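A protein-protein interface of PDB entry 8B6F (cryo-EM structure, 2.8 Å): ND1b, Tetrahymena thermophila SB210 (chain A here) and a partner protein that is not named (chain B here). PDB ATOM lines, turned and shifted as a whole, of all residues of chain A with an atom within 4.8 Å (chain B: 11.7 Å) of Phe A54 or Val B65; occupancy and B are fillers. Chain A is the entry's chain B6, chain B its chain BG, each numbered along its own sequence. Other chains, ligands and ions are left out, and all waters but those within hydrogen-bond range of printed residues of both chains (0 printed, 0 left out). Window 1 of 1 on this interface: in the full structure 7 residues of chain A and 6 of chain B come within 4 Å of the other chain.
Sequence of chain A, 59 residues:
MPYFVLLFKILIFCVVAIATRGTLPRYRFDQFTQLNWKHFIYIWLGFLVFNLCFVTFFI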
ATOM      1  N   PHE A  50     -17.109  -9.077  -9.230  1.00  0.00           N
ATOM      2  CA  PHE A  50     -18.192  -9.855  -9.819  1.00  0.00           C
ATOM      3  C   PHE A  50     -18.319  -9.567 -11.310  1.00  0.00           C
ATOM      4  O   PHE A  50     -18.529 -10.485 -12.110  1.00  0.00           O
ATOM      5  CB  PHE A  50     -19.508  -9.556  -9.101  1.00  0.00           C
ATOM      6  CG  PHE A  50     -19.817 -10.506  -7.979  1.00  0.00           C
ATOM      7  CD1 PHE A  50     -19.359 -10.259  -6.696  1.00  0.00           C
ATOM      8  CD2 PHE A  50     -20.574 -11.643  -8.208  1.00  0.00           C
ATOM      9  CE1 PHE A  50     -19.644 -11.132  -5.663  1.00  0.00           C
ATOM     10  CE2 PHE A  50     -20.862 -12.519  -7.180  1.00  0.00           C
ATOM     11  CZ  PHE A  50     -20.397 -12.262  -5.905  1.00  0.00           C
ATOM     12  N   ASN A  51     -18.197  -8.298 -11.702  1.00  0.00           N
ATOM     13  CA  ASN A  51     -18.245  -7.965 -13.122  1.00  0.00           C
ATOM     14  C   ASN A  51     -17.090  -8.611 -13.870  1.00  0.00           C
ATOM     15  O   ASN A  51     -17.271  -9.135 -14.974  1.00  0.00           O
ATOM     16  CB  ASN A  51     -18.222  -6.450 -13.313  1.00  0.00           C
ATOM     17  CG  ASN A  51     -19.584  -5.818 -13.132  1.00  0.00           C
ATOM     18  OD1 ASN A  51     -20.598  -6.510 -13.056  1.00  0.00           O
ATOM     19  ND2 ASN A  51     -19.616  -4.492 -13.079  1.00  0.00           N
ATOM     20  N   LEU A  52     -15.890  -8.581 -13.287  1.00  0.00           N
ATOM     21  CA  LEU A  52     -14.750  -9.233 -13.924  1.00  0.00           C
ATOM     22  C   LEU A  52     -15.003 -10.723 -14.092  1.00  0.00           C
ATOM     23  O   LEU A  52     -14.719 -11.296 -15.149  1.00  0.00           O
ATOM     24  CB  LEU A  52     -13.485  -9.001 -13.098  1.00  0.00           C
ATOM     25  CG  LEU A  52     -12.943  -7.572 -13.054  1.00  0.00           C
ATOM     26  CD1 LEU A  52     -11.983  -7.398 -11.896  1.00  0.00           C
ATOM     27  CD2 LEU A  52     -12.229  -7.268 -14.338  1.00  0.00           C
ATOM     28  N   CYS A  53     -15.531 -11.370 -13.052  1.00  0.00           N
ATOM     29  CA  CYS A  53     -15.807 -12.798 -13.133  1.00  0.00           C
ATOM     30  C   CYS A  53     -16.851 -13.109 -14.200  1.00  0.00           C
ATOM     31  O   CYS A  53     -16.699 -14.067 -14.966  1.00  0.00           O
ATOM     32  CB  CYS A  53     -16.267 -13.306 -11.767  1.00  0.00           C
ATOM     33  SG  CYS A  53     -14.962 -13.363 -10.524  1.00  0.00           S
ATOM     34  N   PHE A  54     -17.920 -12.311 -14.265  1.00  0.00           N
ATOM     35  CA  PHE A  54     -18.954 -12.551 -15.269  1.00  0.00           C
ATOM     36  C   PHE A  54     -18.425 -12.338 -16.682  1.00  0.00           C
ATOM     37  O   PHE A  54     -18.745 -13.112 -17.591  1.00  0.00           O
ATOM     38  CB  PHE A  54     -20.159 -11.647 -15.009  1.00  0.00           C
ATOM     39  CG  PHE A  54     -20.921 -11.990 -13.756  1.00  0.00           C
ATOM     40  CD1 PHE A  54     -21.070 -13.306 -13.349  1.00  0.00           C
ATOM     41  CD2 PHE A  54     -21.489 -10.990 -12.988  1.00  0.00           C
ATOM     42  CE1 PHE A  54     -21.769 -13.616 -12.201  1.00  0.00           C
ATOM     43  CE2 PHE A  54     -22.190 -11.295 -11.839  1.00  0.00           C
ATOM     44  CZ  PHE A  54     -22.330 -12.609 -11.445  1.00  0.00           C
ATOM     45  N   VAL A  55     -17.615 -11.301 -16.889  1.00  0.00           N
ATOM     46  CA  VAL A  55     -17.051 -11.059 -18.215  1.00  0.00           C
ATOM     47  C   VAL A  55     -16.131 -12.201 -18.613  1.00  0.00           C
ATOM     48  O   VAL A  55     -16.126 -12.643 -19.767  1.00  0.00           O
ATOM     49  CB  VAL A  55     -16.329  -9.698 -18.252  1.00  0.00           C
ATOM     50  CG1 VAL A  55     -15.436  -9.579 -19.481  1.00  0.00           C
ATOM     51  CG2 VAL A  55     -17.346  -8.580 -18.249  1.00  0.00           C
ATOM     52  N   THR A  56     -15.334 -12.692 -17.667  1.00  0.00           N
ATOM     53  CA  THR A  56     -14.482 -13.839 -17.952  1.00  0.00           C
ATOM     54  C   THR A  56     -15.320 -15.062 -18.299  1.00  0.00           C
ATOM     55  O   THR A  56     -14.969 -15.829 -19.204  1.00  0.00           O
ATOM     56  CB  THR A  56     -13.580 -14.123 -16.755  1.00  0.00           C
ATOM     57  OG1 THR A  56     -12.820 -12.951 -16.433  1.00  0.00           O
ATOM     58  CG2 THR A  56     -12.620 -15.227 -17.083  1.00  0.00           C
ATOM     59  N   PHE A  57     -16.424 -15.270 -17.581  1.00  0.00           N
ATOM     60  CA  PHE A  57     -17.295 -16.407 -17.860  1.00  0.00           C
ATOM     61  C   PHE A  57     -17.887 -16.321 -19.261  1.00  0.00           C
ATOM     62  O   PHE A  57     -17.926 -17.320 -19.988  1.00  0.00           O
ATOM     63  CB  PHE A  57     -18.405 -16.471 -16.808  1.00  0.00           C
ATOM     64  CG  PHE A  57     -19.491 -17.461 -17.121  1.00  0.00           C
ATOM     65  CD1 PHE A  57     -20.580 -17.095 -17.896  1.00  0.00           C
ATOM     66  CD2 PHE A  57     -19.442 -18.747 -16.612  1.00  0.00           C
ATOM     67  CE1 PHE A  57     -21.584 -17.996 -18.177  1.00  0.00           C
ATOM     68  CE2 PHE A  57     -20.445 -19.654 -16.890  1.00  0.00           C
ATOM     69  CZ  PHE A  57     -21.518 -19.278 -17.673  1.00  0.00           C
ATOM     70  N   PHE A  58     -18.358 -15.139 -19.658  1.00  0.00           N
ATOM     71  CA  PHE A  58     -19.020 -14.999 -20.949  1.00  0.00           C
ATOM     72  C   PHE A  58     -18.033 -14.989 -22.108  1.00  0.00           C
ATOM     73  O   PHE A  58     -18.354 -15.494 -23.188  1.00  0.00           O
ATOM     74  CB  PHE A  58     -19.871 -13.728 -20.969  1.00  0.00           C
ATOM     75  CG  PHE A  58     -21.174 -13.864 -20.238  1.00  0.00           C
ATOM     76  CD1 PHE A  58     -22.201 -14.629 -20.764  1.00  0.00           C
ATOM     77  CD2 PHE A  58     -21.373 -13.227 -19.026  1.00  0.00           C
ATOM     78  CE1 PHE A  58     -23.401 -14.757 -20.095  1.00  0.00           C
ATOM     79  CE2 PHE A  58     -22.571 -13.352 -18.349  1.00  0.00           C
ATOM     80  CZ  PHE A  58     -23.586 -14.118 -18.885  1.00  0.00           C
ATOM     81  N   LEU B  54     -32.016  -8.850  -3.824  1.00  0.00           N
ATOM     82  CA  LEU B  54     -30.648  -9.331  -3.977  1.00  0.00           C
ATOM     83  C   LEU B  54     -30.547 -10.361  -5.094  1.00  0.00           C
ATOM     84  O   LEU B  54     -29.641 -10.297  -5.930  1.00  0.00           O
ATOM     85  CB  LEU B  54     -30.139  -9.908  -2.656  1.00  0.00           C
ATOM     86  CG  LEU B  54     -29.920  -8.892  -1.529  1.00  0.00           C
ATOM     87  CD1 LEU B  54     -29.509  -9.594  -0.251  1.00  0.00           C
ATOM     88  CD2 LEU B  54     -28.882  -7.848  -1.910  1.00  0.00           C
ATOM     89  N   ALA B  55     -31.464 -11.330  -5.120  1.00  0.00           N
ATOM     90  CA  ALA B  55     -31.429 -12.325  -6.185  1.00  0.00           C
ATOM     91  C   ALA B  55     -31.654 -11.676  -7.543  1.00  0.00           C
ATOM     92  O   ALA B  55     -30.960 -11.990  -8.516  1.00  0.00           O
ATOM     93  CB  ALA B  55     -32.475 -13.408  -5.931  1.00  0.00           C
ATOM     94  N   ALA B  56     -32.621 -10.761  -7.624  1.00  0.00           N
ATOM     95  CA  ALA B  56     -32.888 -10.081  -8.885  1.00  0.00           C
ATOM     96  C   ALA B  56     -31.683  -9.270  -9.333  1.00  0.00           C
ATOM     97  O   ALA B  56     -31.343  -9.247 -10.520  1.00  0.00           O
ATOM     98  CB  ALA B  56     -34.117  -9.182  -8.746  1.00  0.00           C
ATOM     99  N   SER B  57     -31.021  -8.598  -8.391  1.00  0.00           N
ATOM    100  CA  SER B  57     -29.849  -7.807  -8.736  1.00  0.00           C
ATOM    101  C   SER B  57     -28.719  -8.688  -9.248  1.00  0.00           C
ATOM    102  O   SER B  57     -28.053  -8.346 -10.231  1.00  0.00           O
ATOM    103  CB  SER B  57     -29.388  -7.009  -7.517  1.00  0.00           C
ATOM    104  OG  SER B  57     -30.390  -6.096  -7.100  1.00  0.00           O
ATOM    105  N   LEU B  58     -28.479  -9.823  -8.590  1.00  0.00           N
ATOM    106  CA  LEU B  58     -27.418 -10.716  -9.040  1.00  0.00           C
ATOM    107  C   LEU B  58     -27.693 -11.227 -10.448  1.00  0.00           C
ATOM    108  O   LEU B  58     -26.815 -11.192 -11.317  1.00  0.00           O
ATOM    109  CB  LEU B  58     -27.271 -11.879  -8.059  1.00  0.00           C
ATOM    110  CG  LEU B  58     -26.201 -12.921  -8.387  1.00  0.00           C
ATOM    111  CD1 LEU B  58     -24.820 -12.292  -8.436  1.00  0.00           C
ATOM    112  CD2 LEU B  58     -26.238 -14.047  -7.368  1.00  0.00           C
ATOM    113  N   LEU B  59     -28.912 -11.712 -10.692  1.00  0.00           N
ATOM    114  CA  LEU B  59     -29.240 -12.245 -12.010  1.00  0.00           C
ATOM    115  C   LEU B  59     -29.243 -11.148 -13.064  1.00  0.00           C
ATOM    116  O   LEU B  59     -28.835 -11.377 -14.209  1.00  0.00           O
ATOM    117  CB  LEU B  59     -30.585 -12.966 -11.969  1.00  0.00           C
ATOM    118  CG  LEU B  59     -30.469 -14.463 -11.675  1.00  0.00           C
ATOM    119  CD1 LEU B  59     -29.787 -14.700 -10.338  1.00  0.00           C
ATOM    120  CD2 LEU B  59     -31.829 -15.129 -11.704  1.00  0.00           C
ATOM    121  N   LEU B  60     -29.703  -9.948 -12.703  1.00  0.00           N
ATOM    122  CA  LEU B  60     -29.656  -8.836 -13.643  1.00  0.00           C
ATOM    123  C   LEU B  60     -28.221  -8.487 -14.009  1.00  0.00           C
ATOM    124  O   LEU B  60     -27.917  -8.232 -15.179  1.00  0.00           O
ATOM    125  CB  LEU B  60     -30.362  -7.616 -13.050  1.00  0.00           C
ATOM    126  CG  LEU B  60     -31.890  -7.649 -13.039  1.00  0.00           C
ATOM    127  CD1 LEU B  60     -32.425  -6.548 -12.150  1.00  0.00           C
ATOM    128  CD2 LEU B  60     -32.439  -7.504 -14.447  1.00  0.00           C
ATOM    129  N   GLN B  61     -27.321  -8.473 -13.025  1.00  0.00           N
ATOM    130  CA  GLN B  61     -25.921  -8.199 -13.324  1.00  0.00           C
ATOM    131  C   GLN B  61     -25.357  -9.238 -14.282  1.00  0.00           C
ATOM    132  O   GLN B  61     -24.721  -8.896 -15.284  1.00  0.00           O
ATOM    133  CB  GLN B  61     -25.108  -8.166 -12.029  1.00  0.00           C
ATOM    134  CG  GLN B  61     -23.627  -7.881 -12.235  1.00  0.00           C
ATOM    135  CD  GLN B  61     -22.840  -7.944 -10.943  1.00  0.00           C
ATOM    136  OE1 GLN B  61     -23.382  -8.266  -9.888  1.00  0.00           O
ATOM    137  NE2 GLN B  61     -21.551  -7.639 -11.022  1.00  0.00           N
ATOM    138  N   MET B  62     -25.589 -10.519 -13.994  1.00  0.00           N
ATOM    139  CA  MET B  62     -25.055 -11.572 -14.849  1.00  0.00           C
ATOM    140  C   MET B  62     -25.632 -11.469 -16.255  1.00  0.00           C
ATOM    141  O   MET B  62     -24.906 -11.580 -17.249  1.00  0.00           O
ATOM    142  CB  MET B  62     -25.339 -12.940 -14.234  1.00  0.00           C
ATOM    143  CG  MET B  62     -24.504 -14.057 -14.834  1.00  0.00           C
ATOM    144  SD  MET B  62     -24.756 -15.637 -14.001  1.00  0.00           S
ATOM    145  CE  MET B  62     -23.580 -16.667 -14.871  1.00  0.00           C
ATOM    146  N   TRP B  63     -26.949 -11.269 -16.354  1.00  0.00           N
ATOM    147  CA  TRP B  63     -27.601 -11.205 -17.658  1.00  0.00           C
ATOM    148  C   TRP B  63     -27.157  -9.977 -18.440  1.00  0.00           C
ATOM    149  O   TRP B  63     -26.957 -10.049 -19.657  1.00  0.00           O
ATOM    150  CB  TRP B  63     -29.121 -11.209 -17.484  1.00  0.00           C
ATOM    151  CG  TRP B  63     -29.877 -11.124 -18.775  1.00  0.00           C
ATOM    152  CD1 TRP B  63     -30.134 -12.144 -19.643  1.00  0.00           C
ATOM    153  CD2 TRP B  63     -30.481  -9.954 -19.341  1.00  0.00           C
ATOM    154  NE1 TRP B  63     -30.856 -11.681 -20.714  1.00  0.00           N
ATOM    155  CE2 TRP B  63     -31.083 -10.340 -20.553  1.00  0.00           C
ATOM    156  CE3 TRP B  63     -30.567  -8.616 -18.939  1.00  0.00           C
ATOM    157  CZ2 TRP B  63     -31.762  -9.438 -21.370  1.00  0.00           C
ATOM    158  CZ3 TRP B  63     -31.243  -7.721 -19.750  1.00  0.00           C
ATOM    159  CH2 TRP B  63     -31.832  -8.136 -20.953  1.00  0.00           C
ATOM    160  N   GLY B  64     -26.998  -8.840 -17.761  1.00  0.00           N
ATOM    161  CA  GLY B  64     -26.539  -7.644 -18.447  1.00  0.00           C
ATOM    162  C   GLY B  64     -25.111  -7.763 -18.941  1.00  0.00           C
ATOM    163  O   GLY B  64     -24.787  -7.308 -20.040  1.00  0.00           O
ATOM    164  N   VAL B  65     -24.237  -8.379 -18.144  1.00  0.00           N
ATOM    165  CA  VAL B  65     -22.872  -8.618 -18.602  1.00  0.00           C
ATOM    166  C   VAL B  65     -22.882  -9.534 -19.817  1.00  0.00           C
ATOM    167  O   VAL B  65     -22.161  -9.302 -20.794  1.00  0.00           O
ATOM    168  CB  VAL B  65     -22.014  -9.193 -17.459  1.00  0.00           C
ATOM    169  CG1 VAL B  65     -20.645  -9.620 -17.973  1.00  0.00           C
ATOM    170  CG2 VAL B  65     -21.855  -8.168 -16.354  1.00  0.00           C
ATOM    171  N   GLY B  66     -23.701 -10.584 -19.780  1.00  0.00           N
ATOM    172  CA  GLY B  66     -23.819 -11.455 -20.937  1.00  0.00           C
ATOM    173  C   GLY B  66     -24.297 -10.713 -22.168  1.00  0.00           C
ATOM    174  O   GLY B  66     -23.801 -10.939 -23.273  1.00  0.00           O
ATOM    175  N   LYS B  67     -25.276  -9.824 -21.996  1.00  0.00           N
ATOM    176  CA  LYS B  67     -25.787  -9.057 -23.127  1.00  0.00           C
ATOM    177  C   LYS B  67     -24.722  -8.122 -23.689  1.00  0.00           C
ATOM    178  O   LYS B  67     -24.598  -7.981 -24.910  1.00  0.00           O
ATOM    179  CB  LYS B  67     -27.027  -8.273 -22.702  1.00  0.00           C
ATOM    180  CG  LYS B  67     -27.728  -7.536 -23.840  1.00  0.00           C
ATOM    181  CD  LYS B  67     -28.253  -8.477 -24.920  1.00  0.00           C
ATOM    182  CE  LYS B  67     -29.273  -9.461 -24.374  1.00  0.00           C
ATOM    183  NZ  LYS B  67     -29.906 -10.254 -25.461  1.00  0.00           N
ATOM    184  N   ILE B  68     -23.943  -7.479 -22.819  1.00  0.00           N
ATOM    185  CA  ILE B  68     -22.880  -6.593 -23.286  1.00  0.00           C
ATOM    186  C   ILE B  68     -21.822  -7.386 -24.039  1.00  0.00           C
ATOM    187  O   ILE B  68     -21.280  -6.921 -25.050  1.00  0.00           O
ATOM    188  CB  ILE B  68     -22.272  -5.815 -22.102  1.00  0.00           C
ATOM    189  CG1 ILE B  68     -23.303  -4.864 -21.484  1.00  0.00           C
ATOM    190  CG2 ILE B  68     -21.032  -5.039 -22.540  1.00  0.00           C
ATOM    191  CD1 ILE B  68     -23.808  -3.778 -22.410  1.00  0.00           C
ATOM    192  N   ILE B  69     -21.500  -8.587 -23.561  1.00  0.00           N
ATOM    193  CA  ILE B  69     -20.546  -9.428 -24.277  1.00  0.00           C
ATOM    194  C   ILE B  69     -21.117  -9.830 -25.629  1.00  0.00           C
ATOM    195  O   ILE B  69     -20.390  -9.909 -26.625  1.00  0.00           O
ATOM    196  CB  ILE B  69     -20.166 -10.655 -23.427  1.00  0.00           C
ATOM    197  CG1 ILE B  69     -19.421 -10.225 -22.159  1.00  0.00           C
ATOM    198  CG2 ILE B  69     -19.317 -11.633 -24.237  1.00  0.00           C
ATOM    199  CD1 ILE B  69     -18.105  -9.517 -22.400  1.00  0.00           C
ATOM    200  N   GLU B  70     -22.423 -10.095 -25.688  1.00  0.00           N
ATOM    201  CA  GLU B  70     -23.052 -10.399 -26.968  1.00  0.00           C
ATOM    202  C   GLU B  70     -22.907  -9.230 -27.931  1.00  0.00           C
ATOM    203  O   GLU B  70     -22.599  -9.420 -29.112  1.00  0.00           O
ATOM    204  CB  GLU B  70     -24.526 -10.740 -26.751  1.00  0.00           C
ATOM    205  CG  GLU B  70     -25.275 -11.163 -28.007  1.00  0.00           C
ATOM    206  CD  GLU B  70     -24.916 -12.564 -28.464  1.00  0.00           C
ATOM    207  OE1 GLU B  70     -24.579 -13.407 -27.605  1.00  0.00           O
ATOM    208  OE2 GLU B  70     -24.973 -12.824 -29.685  1.00  0.00           O
ATOM    209  N   ILE B  71     -23.143  -8.008 -27.447  1.00  0.00           N
ATOM    210  CA  ILE B  71     -23.000  -6.828 -28.294  1.00  0.00           C
ATOM    211  C   ILE B  71     -21.560  -6.681 -28.766  1.00  0.00           C
ATOM    212  O   ILE B  71     -21.303  -6.400 -29.942  1.00  0.00           O
ATOM    213  CB  ILE B  71     -23.476  -5.572 -27.540  1.00  0.00           C
ATOM    214  CG1 ILE B  71     -24.963  -5.688 -27.206  1.00  0.00           C
ATOM    215  CG2 ILE B  71     -23.230  -4.320 -28.372  1.00  0.00           C
ATOM    216  CD1 ILE B  71     -25.459  -4.638 -26.237  1.00  0.00           C
ATOM    217  N   LYS B  72     -20.599  -6.868 -27.859  1.00  0.00           N
ATOM    218  CA  LYS B  72     -19.194  -6.749 -28.238  1.00  0.00           C
ATOM    219  C   LYS B  72     -18.813  -7.776 -29.293  1.00  0.00           C
ATOM    220  O   LYS B  72     -18.083  -7.463 -30.239  1.00  0.00           O
ATOM    221  CB  LYS B  72     -18.305  -6.900 -27.005  1.00  0.00           C
ATOM    222  CG  LYS B  72     -18.249  -5.669 -26.117  1.00  0.00           C
ATOM    223  CD  LYS B  72     -17.232  -5.848 -24.998  1.00  0.00           C
ATOM    224  CE  LYS B  72     -16.980  -4.546 -24.255  1.00  0.00           C
ATOM    225  NZ  LYS B  72     -18.195  -4.052 -23.557  1.00  0.00           N
ATOM    226  N   LYS B  73     -19.292  -9.011 -29.147  1.00  0.00           N
ATOM    227  CA  LYS B  73     -18.956 -10.044 -30.119  1.00  0.00           C
ATOM    228  C   LYS B  73     -19.613  -9.786 -31.467  1.00  0.00           C
ATOM    229  O   LYS B  73     -19.023 -10.092 -32.508  1.00  0.00           O
ATOM    230  CB  LYS B  73     -19.349 -11.416 -29.577  1.00  0.00           C
ATOM    231  CG  LYS B  73     -18.574 -11.816 -28.330  1.00  0.00           C
ATOM    232  CD  LYS B  73     -17.114 -12.103 -28.640  1.00  0.00           C
ATOM    233  CE  LYS B  73     -16.377 -12.568 -27.396  1.00  0.00           C
ATOM    234  NZ  LYS B  73     -14.953 -12.889 -27.682  1.00  0.00           N
ATOM    235  N   PHE B  74     -20.830  -9.236 -31.476  1.00  0.00           N
ATOM    236  CA  PHE B  74     -21.434  -8.824 -32.739  1.00  0.00           C
ATOM    237  C   PHE B  74     -20.616  -7.721 -33.396  1.00  0.00           C
ATOM    238  O   PHE B  74     -20.399  -7.738 -34.613  1.00  0.00           O
ATOM    239  CB  PHE B  74     -22.872  -8.362 -32.501  1.00  0.00           C
ATOM    240  CG  PHE B  74     -23.607  -7.999 -33.757  1.00  0.00           C
ATOM    241  CD1 PHE B  74     -24.161  -8.982 -34.560  1.00  0.00           C
ATOM    242  CD2 PHE B  74     -23.759  -6.673 -34.128  1.00  0.00           C
ATOM    243  CE1 PHE B  74     -24.845  -8.650 -35.715  1.00  0.00           C
ATOM    244  CE2 PHE B  74     -24.442  -6.335 -35.280  1.00  0.00           C
ATOM    245  CZ  PHE B  74     -24.986  -7.323 -36.075  1.00  0.00           C
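The side-chain amide nitrogen (NE2) of Gln B61 sits at hydrogen-bond distance from the side-chain amide oxygen (OD1) of Asn A51 (2.5 Å).
Printed residues of chain B that touch a printed residue of chain A: Leu B58, Gln B61, Met B62, Val B65, Gly B66 and Ile B69.
Hydrophobic or aromatic side chains of chain B that line the printed part of chain A: Leu B58, Met B62, Val B65 and Ile B69.
Printed residues of chain A that touch a printed residue of chain B: Phe A50, Asn A51, Phe A54, Val A55 and Phe A58.
Hydrophobic or aromatic side chains of chain A that line the printed part of chain B: Phe A50, Phe A54, Val A55 and Phe A58.
Among the printed residues, 13 pairs touch across the chains.
Among the printed residues, merely in contact across the chains: Phe A50 with Gln B61 (3.4 Å), Asn A51 with Val B65 (3.9 Å), Phe A54 with Leu B58 (3.9 Å), Phe A54 with Gln B61 (3.5 Å), Phe A54 with Met B62 (3.8 Å), Phe A54 with Val B65 (3.6 Å), Val A55 with Val B65 (3.5 Å), Val A55 with Ile B69 (3.96 Å), Phe A58 with Met B62 (3.1 Å), Phe A58 with Val B65 (3.8 Å), Phe A58 with Gly B66 (3.3 Å) and Phe A58 with Ile B69 (3.7 Å).
Asn A51 touches just these residues of chain B: Gln B61 and Val B65.
No residue of chain B comes within 4 Å of Cys A53.
Printed residues of chain B within 4 Å of Phe A54: Leu B58, Gln B61, Met B62 and Val B65.
Val A55 touches just these residues of chain B: Val B65 and Ile B69.
No residue of chain B comes within 4 Å of Thr A56.
No residue of chain B comes within 4 Å of Phe A57.
Of chain B, only Met B62 (3.1 Å), Val B65 (3.8 Å), Gly B66 (3.3 Å) and Ile B69 (3.7 Å) come within 4 Å of Phe A58.
Of the printed residues of chain A, Leu B58 touches Phe A54 (3.9 Å).
Of the printed residues of chain A, Gln B61 touches Phe A50 (3.4 Å), Asn A51 (2.5 Å) and Phe A54 (3.5 Å).
Of the printed residues of chain A, Met B62 touches Phe A54 and Phe A58.
Of the printed residues of chain A, Gly B66 touches Phe A58 (3.3 Å).
Of the printed residues of chain A, Ile B69 touches Val A55 (3.96 Å) and Phe A58 (3.7 Å).
The nearest residue of chain B that does not touch Phe A54 is Ile B69 (5.4 Å).
The nearest printed residue of chain A that does not touch Val B65 is Phe A50 (5.9 Å).
The nearest printed residue of chain A that does not touch Gly B66 is Phe A54 (6.0 Å).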
